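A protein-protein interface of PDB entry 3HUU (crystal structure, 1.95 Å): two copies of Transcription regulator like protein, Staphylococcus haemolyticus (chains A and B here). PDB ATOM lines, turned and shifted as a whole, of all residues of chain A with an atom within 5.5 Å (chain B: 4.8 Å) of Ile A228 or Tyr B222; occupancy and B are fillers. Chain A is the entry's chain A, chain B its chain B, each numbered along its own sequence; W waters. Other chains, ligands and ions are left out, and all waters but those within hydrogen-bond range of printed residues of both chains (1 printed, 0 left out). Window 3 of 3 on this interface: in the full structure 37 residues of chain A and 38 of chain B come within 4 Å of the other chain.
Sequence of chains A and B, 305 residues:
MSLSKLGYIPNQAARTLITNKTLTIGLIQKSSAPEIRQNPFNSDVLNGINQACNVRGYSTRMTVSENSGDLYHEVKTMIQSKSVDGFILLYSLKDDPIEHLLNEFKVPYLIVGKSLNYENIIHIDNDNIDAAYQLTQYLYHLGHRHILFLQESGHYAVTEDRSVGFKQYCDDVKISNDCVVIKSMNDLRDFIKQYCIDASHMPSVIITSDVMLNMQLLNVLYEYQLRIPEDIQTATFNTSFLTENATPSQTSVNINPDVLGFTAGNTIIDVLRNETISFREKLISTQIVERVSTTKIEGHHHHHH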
ATOM      1  N   LEU A 218     -13.755 -16.966 -21.601  1.00  0.00           N
ATOM      2  CA  LEU A 218     -13.858 -15.939 -22.645  1.00  0.00           C
ATOM      3  C   LEU A 218     -14.793 -14.827 -22.179  1.00  0.00           C
ATOM      4  O   LEU A 218     -14.596 -13.655 -22.508  1.00  0.00           O
ATOM      5  CB  LEU A 218     -14.379 -16.543 -23.957  1.00  0.00           C
ATOM      6  CG  LEU A 218     -13.554 -17.684 -24.568  1.00  0.00           C
ATOM      7  CD1 LEU A 218     -14.238 -18.170 -25.845  1.00  0.00           C
ATOM      8  CD2 LEU A 218     -12.142 -17.222 -24.879  1.00  0.00           C
ATOM      9  N   LEU A 221     -12.738 -12.690 -19.685  1.00  0.00           N
ATOM     10  CA  LEU A 221     -11.721 -11.918 -20.396  1.00  0.00           C
ATOM     11  C   LEU A 221     -12.343 -10.731 -21.141  1.00  0.00           C
ATOM     12  O   LEU A 221     -11.744  -9.649 -21.222  1.00  0.00           O
ATOM     13  CB  LEU A 221     -10.950 -12.823 -21.376  1.00  0.00           C
ATOM     14  CG  LEU A 221     -10.029 -13.883 -20.751  1.00  0.00           C
ATOM     15  CD1 LEU A 221      -9.518 -14.848 -21.823  1.00  0.00           C
ATOM     16  CD2 LEU A 221      -8.856 -13.202 -20.051  1.00  0.00           C
ATOM     17  N   TYR A 222     -13.539 -10.932 -21.692  1.00  0.00           N
ATOM     18  CA  TYR A 222     -14.244  -9.869 -22.409  1.00  0.00           C
ATOM     19  C   TYR A 222     -14.636  -8.761 -21.430  1.00  0.00           C
ATOM     20  O   TYR A 222     -14.455  -7.573 -21.712  1.00  0.00           O
ATOM     21  CB  TYR A 222     -15.514 -10.417 -23.060  1.00  0.00           C
ATOM     22  CG  TYR A 222     -16.246  -9.444 -23.965  1.00  0.00           C
ATOM     23  CD1 TYR A 222     -15.829  -9.235 -25.278  1.00  0.00           C
ATOM     24  CD2 TYR A 222     -17.410  -8.804 -23.537  1.00  0.00           C
ATOM     25  CE1 TYR A 222     -16.564  -8.427 -26.152  1.00  0.00           C
ATOM     26  CE2 TYR A 222     -18.152  -7.987 -24.402  1.00  0.00           C
ATOM     27  CZ  TYR A 222     -17.727  -7.810 -25.710  1.00  0.00           C
ATOM     28  OH  TYR A 222     -18.485  -7.071 -26.595  1.00  0.00           O
ATOM     29  N   LEU A 226      -9.783  -7.846 -22.108  1.00  0.00           N
ATOM     30  CA  LEU A 226      -8.506  -8.398 -22.550  1.00  0.00           C
ATOM     31  C   LEU A 226      -8.771  -9.034 -23.911  1.00  0.00           C
ATOM     32  O   LEU A 226      -9.442 -10.061 -24.003  1.00  0.00           O
ATOM     33  CB  LEU A 226      -8.003  -9.439 -21.543  1.00  0.00           C
ATOM     34  CG  LEU A 226      -7.667  -8.882 -20.155  1.00  0.00           C
ATOM     35  CD1 LEU A 226      -7.390 -10.014 -19.186  1.00  0.00           C
ATOM     36  CD2 LEU A 226      -6.465  -7.949 -20.253  1.00  0.00           C
ATOM     37  N   ARG A 227      -8.255  -8.408 -24.964  1.00  0.00           N
ATOM     38  CA  ARG A 227      -8.454  -8.890 -26.326  1.00  0.00           C
ATOM     39  C   ARG A 227      -7.660 -10.154 -26.627  1.00  0.00           C
ATOM     40  O   ARG A 227      -6.554 -10.344 -26.116  1.00  0.00           O
ATOM     41  CB  ARG A 227      -8.074  -7.799 -27.337  1.00  0.00           C
ATOM     42  CG  ARG A 227      -8.609  -8.047 -28.742  1.00  0.00           C
ATOM     43  CD  ARG A 227     -10.104  -7.738 -28.821  1.00  0.00           C
ATOM     44  NE  ARG A 227     -10.722  -8.216 -30.058  1.00  0.00           N
ATOM     45  CZ  ARG A 227     -10.336  -7.869 -31.281  1.00  0.00           C
ATOM     46  NH1 ARG A 227      -9.321  -7.031 -31.448  1.00  0.00           N
ATOM     47  NH2 ARG A 227     -10.960  -8.367 -32.340  1.00  0.00           N
ATOM     48  N   ILE A 228      -8.238 -11.010 -27.468  1.00  0.00           N
ATOM     49  CA  ILE A 228      -7.618 -12.268 -27.866  1.00  0.00           C
ATOM     50  C   ILE A 228      -7.447 -12.246 -29.371  1.00  0.00           C
ATOM     51  O   ILE A 228      -8.395 -11.972 -30.093  1.00  0.00           O
ATOM     52  CB  ILE A 228      -8.517 -13.472 -27.507  1.00  0.00           C
ATOM     53  CG1 ILE A 228      -8.837 -13.443 -26.010  1.00  0.00           C
ATOM     54  CG2 ILE A 228      -7.817 -14.780 -27.889  1.00  0.00           C
ATOM     55  CD1 ILE A 228      -9.912 -14.430 -25.594  1.00  0.00           C
ATOM     56  N   PRO A 229      -6.247 -12.565 -29.874  1.00  0.00           N
ATOM     57  CA  PRO A 229      -5.015 -12.969 -29.191  1.00  0.00           C
ATOM     58  C   PRO A 229      -4.059 -11.820 -28.820  1.00  0.00           C
ATOM     59  O   PRO A 229      -3.003 -12.055 -28.237  1.00  0.00           O
ATOM     60  CB  PRO A 229      -4.385 -13.922 -30.197  1.00  0.00           C
ATOM     61  CG  PRO A 229      -4.679 -13.230 -31.490  1.00  0.00           C
ATOM     62  CD  PRO A 229      -6.132 -12.801 -31.327  1.00  0.00           C
ATOM     63  N   GLU A 230      -4.431 -10.587 -29.152  1.00  0.00           N
ATOM     64  CA  GLU A 230      -3.589  -9.426 -28.868  1.00  0.00           C
ATOM     65  C   GLU A 230      -3.078  -9.321 -27.436  1.00  0.00           C
ATOM     66  O   GLU A 230      -1.870  -9.270 -27.209  1.00  0.00           O
ATOM     67  CB  GLU A 230      -4.325  -8.126 -29.222  1.00  0.00           C
ATOM     68  CG  GLU A 230      -4.453  -7.838 -30.716  1.00  0.00           C
ATOM     69  CD  GLU A 230      -5.231  -8.907 -31.464  1.00  0.00           C
ATOM     70  OE1 GLU A 230      -6.331  -9.283 -31.006  1.00  0.00           O
ATOM     71  OE2 GLU A 230      -4.740  -9.361 -32.517  1.00  0.00           O
ATOM     72  N   ASP A 231      -3.991  -9.279 -26.472  1.00  0.00           N
ATOM     73  CA  ASP A 231      -3.600  -9.154 -25.074  1.00  0.00           C
ATOM     74  C   ASP A 231      -3.270 -10.483 -24.402  1.00  0.00           C
ATOM     75  O   ASP A 231      -2.397 -10.547 -23.531  1.00  0.00           O
ATOM     76  CB  ASP A 231      -4.697  -8.439 -24.286  1.00  0.00           C
ATOM     77  CG  ASP A 231      -4.919  -7.011 -24.764  1.00  0.00           C
ATOM     78  OD1 ASP A 231      -3.914  -6.319 -25.035  1.00  0.00           O
ATOM     79  OD2 ASP A 231      -6.086  -6.580 -24.858  1.00  0.00           O
ATOM     80  N   ILE A 232      -3.968 -11.539 -24.803  1.00  0.00           N
ATOM     81  CA  ILE A 232      -3.738 -12.865 -24.226  1.00  0.00           C
ATOM     82  C   ILE A 232      -4.307 -13.921 -25.159  1.00  0.00           C
ATOM     83  O   ILE A 232      -5.225 -13.642 -25.939  1.00  0.00           O
ATOM     84  CB  ILE A 232      -4.410 -12.994 -22.837  1.00  0.00           C
ATOM     85  CG1 ILE A 232      -3.881 -14.233 -22.105  1.00  0.00           C
ATOM     86  CG2 ILE A 232      -5.922 -13.102 -22.987  1.00  0.00           C
ATOM     87  CD1 ILE A 232      -4.300 -14.287 -20.666  1.00  0.00           C
ATOM     88  N   GLN A 233      -3.753 -15.130 -25.088  1.00  0.00           N
ATOM     89  CA  GLN A 233      -4.200 -16.222 -25.939  1.00  0.00           C
ATOM     90  C   GLN A 233      -4.874 -17.308 -25.114  1.00  0.00           C
ATOM     91  O   GLN A 233      -4.684 -17.385 -23.900  1.00  0.00           O
ATOM     92  CB  GLN A 233      -3.010 -16.797 -26.722  1.00  0.00           C
ATOM     93  CG  GLN A 233      -2.415 -15.792 -27.704  1.00  0.00           C
ATOM     94  CD  GLN A 233      -1.237 -16.336 -28.474  1.00  0.00           C
ATOM     95  OE1 GLN A 233      -1.178 -17.532 -28.790  1.00  0.00           O
ATOM     96  NE2 GLN A 233      -0.292 -15.457 -28.805  1.00  0.00           N
ATOM     97  N   THR A 234      -5.671 -18.138 -25.778  1.00  0.00           N
ATOM     98  CA  THR A 234      -6.396 -19.201 -25.092  1.00  0.00           C
ATOM     99  C   THR A 234      -6.500 -20.439 -25.973  1.00  0.00           C
ATOM    100  O   THR A 234      -6.411 -20.362 -27.193  1.00  0.00           O
ATOM    101  CB  THR A 234      -7.835 -18.746 -24.718  1.00  0.00           C
ATOM    102  OG1 THR A 234      -8.544 -18.380 -25.905  1.00  0.00           O
ATOM    103  CG2 THR A 234      -7.801 -17.546 -23.803  1.00  0.00           C
ATOM    104  N   THR A 247     -15.825 -16.566 -29.272  1.00  0.00           N
ATOM    105  CA  THR A 247     -15.406 -15.180 -29.427  1.00  0.00           C
ATOM    106  C   THR A 247     -14.028 -14.970 -28.804  1.00  0.00           C
ATOM    107  O   THR A 247     -13.911 -14.757 -27.595  1.00  0.00           O
ATOM    108  CB  THR A 247     -16.414 -14.231 -28.737  1.00  0.00           C
ATOM    109  OG1 THR A 247     -17.669 -14.291 -29.422  1.00  0.00           O
ATOM    110  CG2 THR A 247     -15.915 -12.801 -28.753  1.00  0.00           C
ATOM    111  N   PRO A 248     -12.961 -15.070 -29.613  1.00  0.00           N
ATOM    112  CA  PRO A 248     -12.926 -15.362 -31.047  1.00  0.00           C
ATOM    113  C   PRO A 248     -12.799 -16.880 -31.208  1.00  0.00           C
ATOM    114  O   PRO A 248     -12.767 -17.592 -30.206  1.00  0.00           O
ATOM    115  CB  PRO A 248     -11.670 -14.631 -31.498  1.00  0.00           C
ATOM    116  CG  PRO A 248     -10.748 -14.956 -30.382  1.00  0.00           C
ATOM    117  CD  PRO A 248     -11.607 -14.723 -29.137  1.00  0.00           C
ATOM    118  N   GLN A 250     -11.665 -20.569 -31.239  1.00  0.00           N
ATOM    119  CA  GLN A 250     -10.680 -21.170 -30.348  1.00  0.00           C
ATOM    120  C   GLN A 250      -9.821 -22.309 -30.881  1.00  0.00           C
ATOM    121  O   GLN A 250     -10.332 -23.283 -31.435  1.00  0.00           O
ATOM    122  CB  GLN A 250     -11.378 -21.696 -29.094  1.00  0.00           C
ATOM    123  CG  GLN A 250     -12.108 -20.655 -28.274  1.00  0.00           C
ATOM    124  CD  GLN A 250     -11.170 -19.629 -27.675  1.00  0.00           C
ATOM    125  OE1 GLN A 250     -11.165 -18.459 -28.073  1.00  0.00           O
ATOM    126  NE2 GLN A 250     -10.373 -20.057 -26.720  1.00  0.00           N
ATOM    127  N   VAL A 292      -8.089 -18.579 -34.483  1.00  0.00           N
ATOM    128  CA  VAL A 292      -7.720 -17.220 -34.109  1.00  0.00           C
ATOM    129  C   VAL A 292      -7.187 -16.982 -32.689  1.00  0.00           C
ATOM    130  O   VAL A 292      -6.376 -16.080 -32.483  1.00  0.00           O
ATOM    131  CB  VAL A 292      -8.932 -16.277 -34.373  1.00  0.00           C
ATOM    132  CG1 VAL A 292      -8.613 -14.847 -33.955  1.00  0.00           C
ATOM    133  CG2 VAL A 292      -9.298 -16.329 -35.849  1.00  0.00           C
ATOM    134  N   SER A 293      -7.607 -17.788 -31.717  1.00  0.00           N
ATOM    135  CA  SER A 293      -7.180 -17.583 -30.334  1.00  0.00           C
ATOM    136  C   SER A 293      -5.686 -17.758 -30.036  1.00  0.00           C
ATOM    137  O   SER A 293      -5.229 -17.367 -28.970  1.00  0.00           O
ATOM    138  CB  SER A 293      -7.991 -18.476 -29.381  1.00  0.00           C
ATOM    139  OG  SER A 293      -7.597 -19.835 -29.481  1.00  0.00           O
ATOM    140  N   LEU B 218     -21.885 -12.914 -32.494  1.00  0.00           N
ATOM    141  CA  LEU B 218     -20.954 -12.373 -31.503  1.00  0.00           C
ATOM    142  C   LEU B 218     -19.509 -12.480 -31.985  1.00  0.00           C
ATOM    143  O   LEU B 218     -18.680 -11.603 -31.724  1.00  0.00           O
ATOM    144  CB  LEU B 218     -21.102 -13.098 -30.168  1.00  0.00           C
ATOM    145  CG  LEU B 218     -22.527 -13.110 -29.613  1.00  0.00           C
ATOM    146  CD1 LEU B 218     -22.535 -13.765 -28.237  1.00  0.00           C
ATOM    147  CD2 LEU B 218     -23.064 -11.689 -29.540  1.00  0.00           C
ATOM    148  N   ASN B 219     -19.221 -13.559 -32.699  1.00  0.00           N
ATOM    149  CA  ASN B 219     -17.893 -13.792 -33.229  1.00  0.00           C
ATOM    150  C   ASN B 219     -17.531 -12.668 -34.200  1.00  0.00           C
ATOM    151  O   ASN B 219     -16.479 -12.033 -34.071  1.00  0.00           O
ATOM    152  CB  ASN B 219     -17.868 -15.159 -33.928  1.00  0.00           C
ATOM    153  CG  ASN B 219     -16.591 -15.394 -34.721  1.00  0.00           C
ATOM    154  OD1 ASN B 219     -16.347 -14.735 -35.736  1.00  0.00           O
ATOM    155  ND2 ASN B 219     -15.775 -16.340 -34.264  1.00  0.00           N
ATOM    156  N   VAL B 220     -18.427 -12.408 -35.147  1.00  0.00           N
ATOM    157  CA  VAL B 220     -18.215 -11.377 -36.153  1.00  0.00           C
ATOM    158  C   VAL B 220     -18.146  -9.967 -35.565  1.00  0.00           C
ATOM    159  O   VAL B 220     -17.333  -9.151 -36.002  1.00  0.00           O
ATOM    160  CB  VAL B 220     -19.307 -11.450 -37.239  1.00  0.00           C
ATOM    161  CG1 VAL B 220     -19.085 -10.376 -38.287  1.00  0.00           C
ATOM    162  CG2 VAL B 220     -19.290 -12.830 -37.891  1.00  0.00           C
ATOM    163  N   LEU B 221     -18.978  -9.677 -34.571  1.00  0.00           N
ATOM    164  CA  LEU B 221     -18.955  -8.358 -33.949  1.00  0.00           C
ATOM    165  C   LEU B 221     -17.634  -8.149 -33.208  1.00  0.00           C
ATOM    166  O   LEU B 221     -17.122  -7.024 -33.135  1.00  0.00           O
ATOM    167  CB  LEU B 221     -20.122  -8.199 -32.972  1.00  0.00           C
ATOM    168  CG  LEU B 221     -21.529  -8.135 -33.564  1.00  0.00           C
ATOM    169  CD1 LEU B 221     -22.558  -8.121 -32.431  1.00  0.00           C
ATOM    170  CD2 LEU B 221     -21.663  -6.878 -34.443  1.00  0.00           C
ATOM    171  N   TYR B 222     -17.096  -9.226 -32.638  1.00  0.00           N
ATOM    172  CA  TYR B 222     -15.827  -9.156 -31.921  1.00  0.00           C
ATOM    173  C   TYR B 222     -14.700  -8.915 -32.928  1.00  0.00           C
ATOM    174  O   TYR B 222     -13.754  -8.181 -32.654  1.00  0.00           O
ATOM    175  CB  TYR B 222     -15.563 -10.462 -31.173  1.00  0.00           C
ATOM    176  CG  TYR B 222     -14.322 -10.456 -30.302  1.00  0.00           C
ATOM    177  CD1 TYR B 222     -14.331  -9.870 -29.043  1.00  0.00           C
ATOM    178  CD2 TYR B 222     -13.160 -11.096 -30.717  1.00  0.00           C
ATOM    179  CE1 TYR B 222     -13.213  -9.935 -28.212  1.00  0.00           C
ATOM    180  CE2 TYR B 222     -12.048 -11.164 -29.903  1.00  0.00           C
ATOM    181  CZ  TYR B 222     -12.077 -10.592 -28.652  1.00  0.00           C
ATOM    182  OH  TYR B 222     -10.988 -10.732 -27.831  1.00  0.00           O
ATOM    183  N   GLU B 223     -14.808  -9.551 -34.089  1.00  0.00           N
ATOM    184  CA  GLU B 223     -13.816  -9.395 -35.142  1.00  0.00           C
ATOM    185  C   GLU B 223     -13.779  -7.942 -35.618  1.00  0.00           C
ATOM    186  O   GLU B 223     -12.708  -7.396 -35.901  1.00  0.00           O
ATOM    187  CB  GLU B 223     -14.152 -10.321 -36.316  1.00  0.00           C
ATOM    188  CG  GLU B 223     -13.331 -10.062 -37.583  1.00  0.00           C
ATOM    189  CD  GLU B 223     -13.713 -10.989 -38.729  1.00  0.00           C
ATOM    190  OE1 GLU B 223     -14.909 -11.323 -38.853  1.00  0.00           O
ATOM    191  OE2 GLU B 223     -12.823 -11.375 -39.515  1.00  0.00           O
ATOM    192  N   TYR B 224     -14.951  -7.317 -35.704  1.00  0.00           N
ATOM    193  CA  TYR B 224     -15.042  -5.933 -36.156  1.00  0.00           C
ATOM    194  C   TYR B 224     -15.041  -4.928 -35.012  1.00  0.00           C
ATOM    195  O   TYR B 224     -15.403  -3.768 -35.192  1.00  0.00           O
ATOM    196  CB  TYR B 224     -16.280  -5.750 -37.037  1.00  0.00           C
ATOM    197  CG  TYR B 224     -16.126  -6.404 -38.387  1.00  0.00           C
ATOM    198  CD1 TYR B 224     -16.271  -7.778 -38.539  1.00  0.00           C
ATOM    199  CD2 TYR B 224     -15.769  -5.655 -39.507  1.00  0.00           C
ATOM    200  CE1 TYR B 224     -16.061  -8.396 -39.775  1.00  0.00           C
ATOM    201  CE2 TYR B 224     -15.555  -6.264 -40.749  1.00  0.00           C
ATOM    202  CZ  TYR B 224     -15.704  -7.636 -40.873  1.00  0.00           C
ATOM    203  OH  TYR B 224     -15.502  -8.249 -42.090  1.00  0.00           O
ATOM    204  N   GLN B 225     -14.634  -5.393 -33.837  1.00  0.00           N
ATOM    205  CA  GLN B 225     -14.537  -4.570 -32.636  1.00  0.00           C
ATOM    206  C   GLN B 225     -15.758  -3.755 -32.227  1.00  0.00           C
ATOM    207  O   GLN B 225     -15.633  -2.612 -31.796  1.00  0.00           O
ATOM    208  CB  GLN B 225     -13.318  -3.653 -32.747  1.00  0.00           C
ATOM    209  CG  GLN B 225     -12.005  -4.415 -32.773  1.00  0.00           C
ATOM    210  CD  GLN B 225     -10.807  -3.510 -32.993  1.00  0.00           C
ATOM    211  OE1 GLN B 225     -10.658  -2.901 -34.052  1.00  0.00           O
ATOM    212  NE2 GLN B 225      -9.949  -3.414 -31.987  1.00  0.00           N
HETATM  213  O   HOH W   1     -11.852 -10.723 -25.138  1.00  0.00           O
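OH of Tyr B222 sits at hydrogen-bond distance from N of Ile A228 (2.8 Å). The guanidinium group of Arg A227 is in hydrogen-bond range of the backbone carbonyl oxygen of Tyr B222 (2.8 Å).
OE1 of Gln A250 lies close to O of Pro A248 (2.8 Å). N of Ile A232 lies within hydrogen-bond range of O of Arg A227, at 3.1 Å. The guanidinium group (NH1) of Arg A227 lies within salt-bridge range of the side-chain carboxylate (OE1) of Glu A230. N of Arg A227 is in hydrogen-bond range of OD2 of Asp A231, at 2.8 Å.
Among the printed residues, merely in contact across the chains: Thr A247 with Tyr B222 (3.2 Å), Thr A247 with Leu B218 (3.6 Å), Pro A248 with Tyr B222 (3.7 Å), Thr A247 with Asn B219 (3.7 Å), Arg A227 with Gln B225 (3.7 Å) and Tyr A222 with Tyr B222 (3.9 Å).
Ile A228 touches just one residue of chain B: Tyr B222. Of the printed residues of chain B, Thr A247 touches Leu B218 (3.6 Å), Asn B219 (3.7 Å) and Tyr B222 (3.2 Å). Of the printed residues of chain B, Pro A248 touches Tyr B222 (3.7 Å). Printed residues of chain A within 4 Å of Asn B219: Thr A247. Tyr B222 touches five residues of chain A. The nearest printed residue of chain B that does not touch Arg A227 is Glu B223 (4.1 Å).
Of the 8 printed residues of chain B, 4 touch a printed residue of chain A. Of the 17 printed residues of chain A, 5 touch a printed residue of chain B. Among the printed residues, 8 pairs touch across the chains. Among the printed residues, no Asp or Glu carboxylate lies within 4 Å of a Lys or Arg side-chain nitrogen of the other chain.
Tyr B222 touches its own counterpart, Tyr A222. Of the 8 pairs that touch across the chains among the printed residues, 1 has its exchanged pair printed and touching as well.
Water W1 bridges the backbone carbonyl oxygen of Leu A226 (2.7 Å) and the side-chain hydroxyl of Tyr B222 (2.8 Å).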
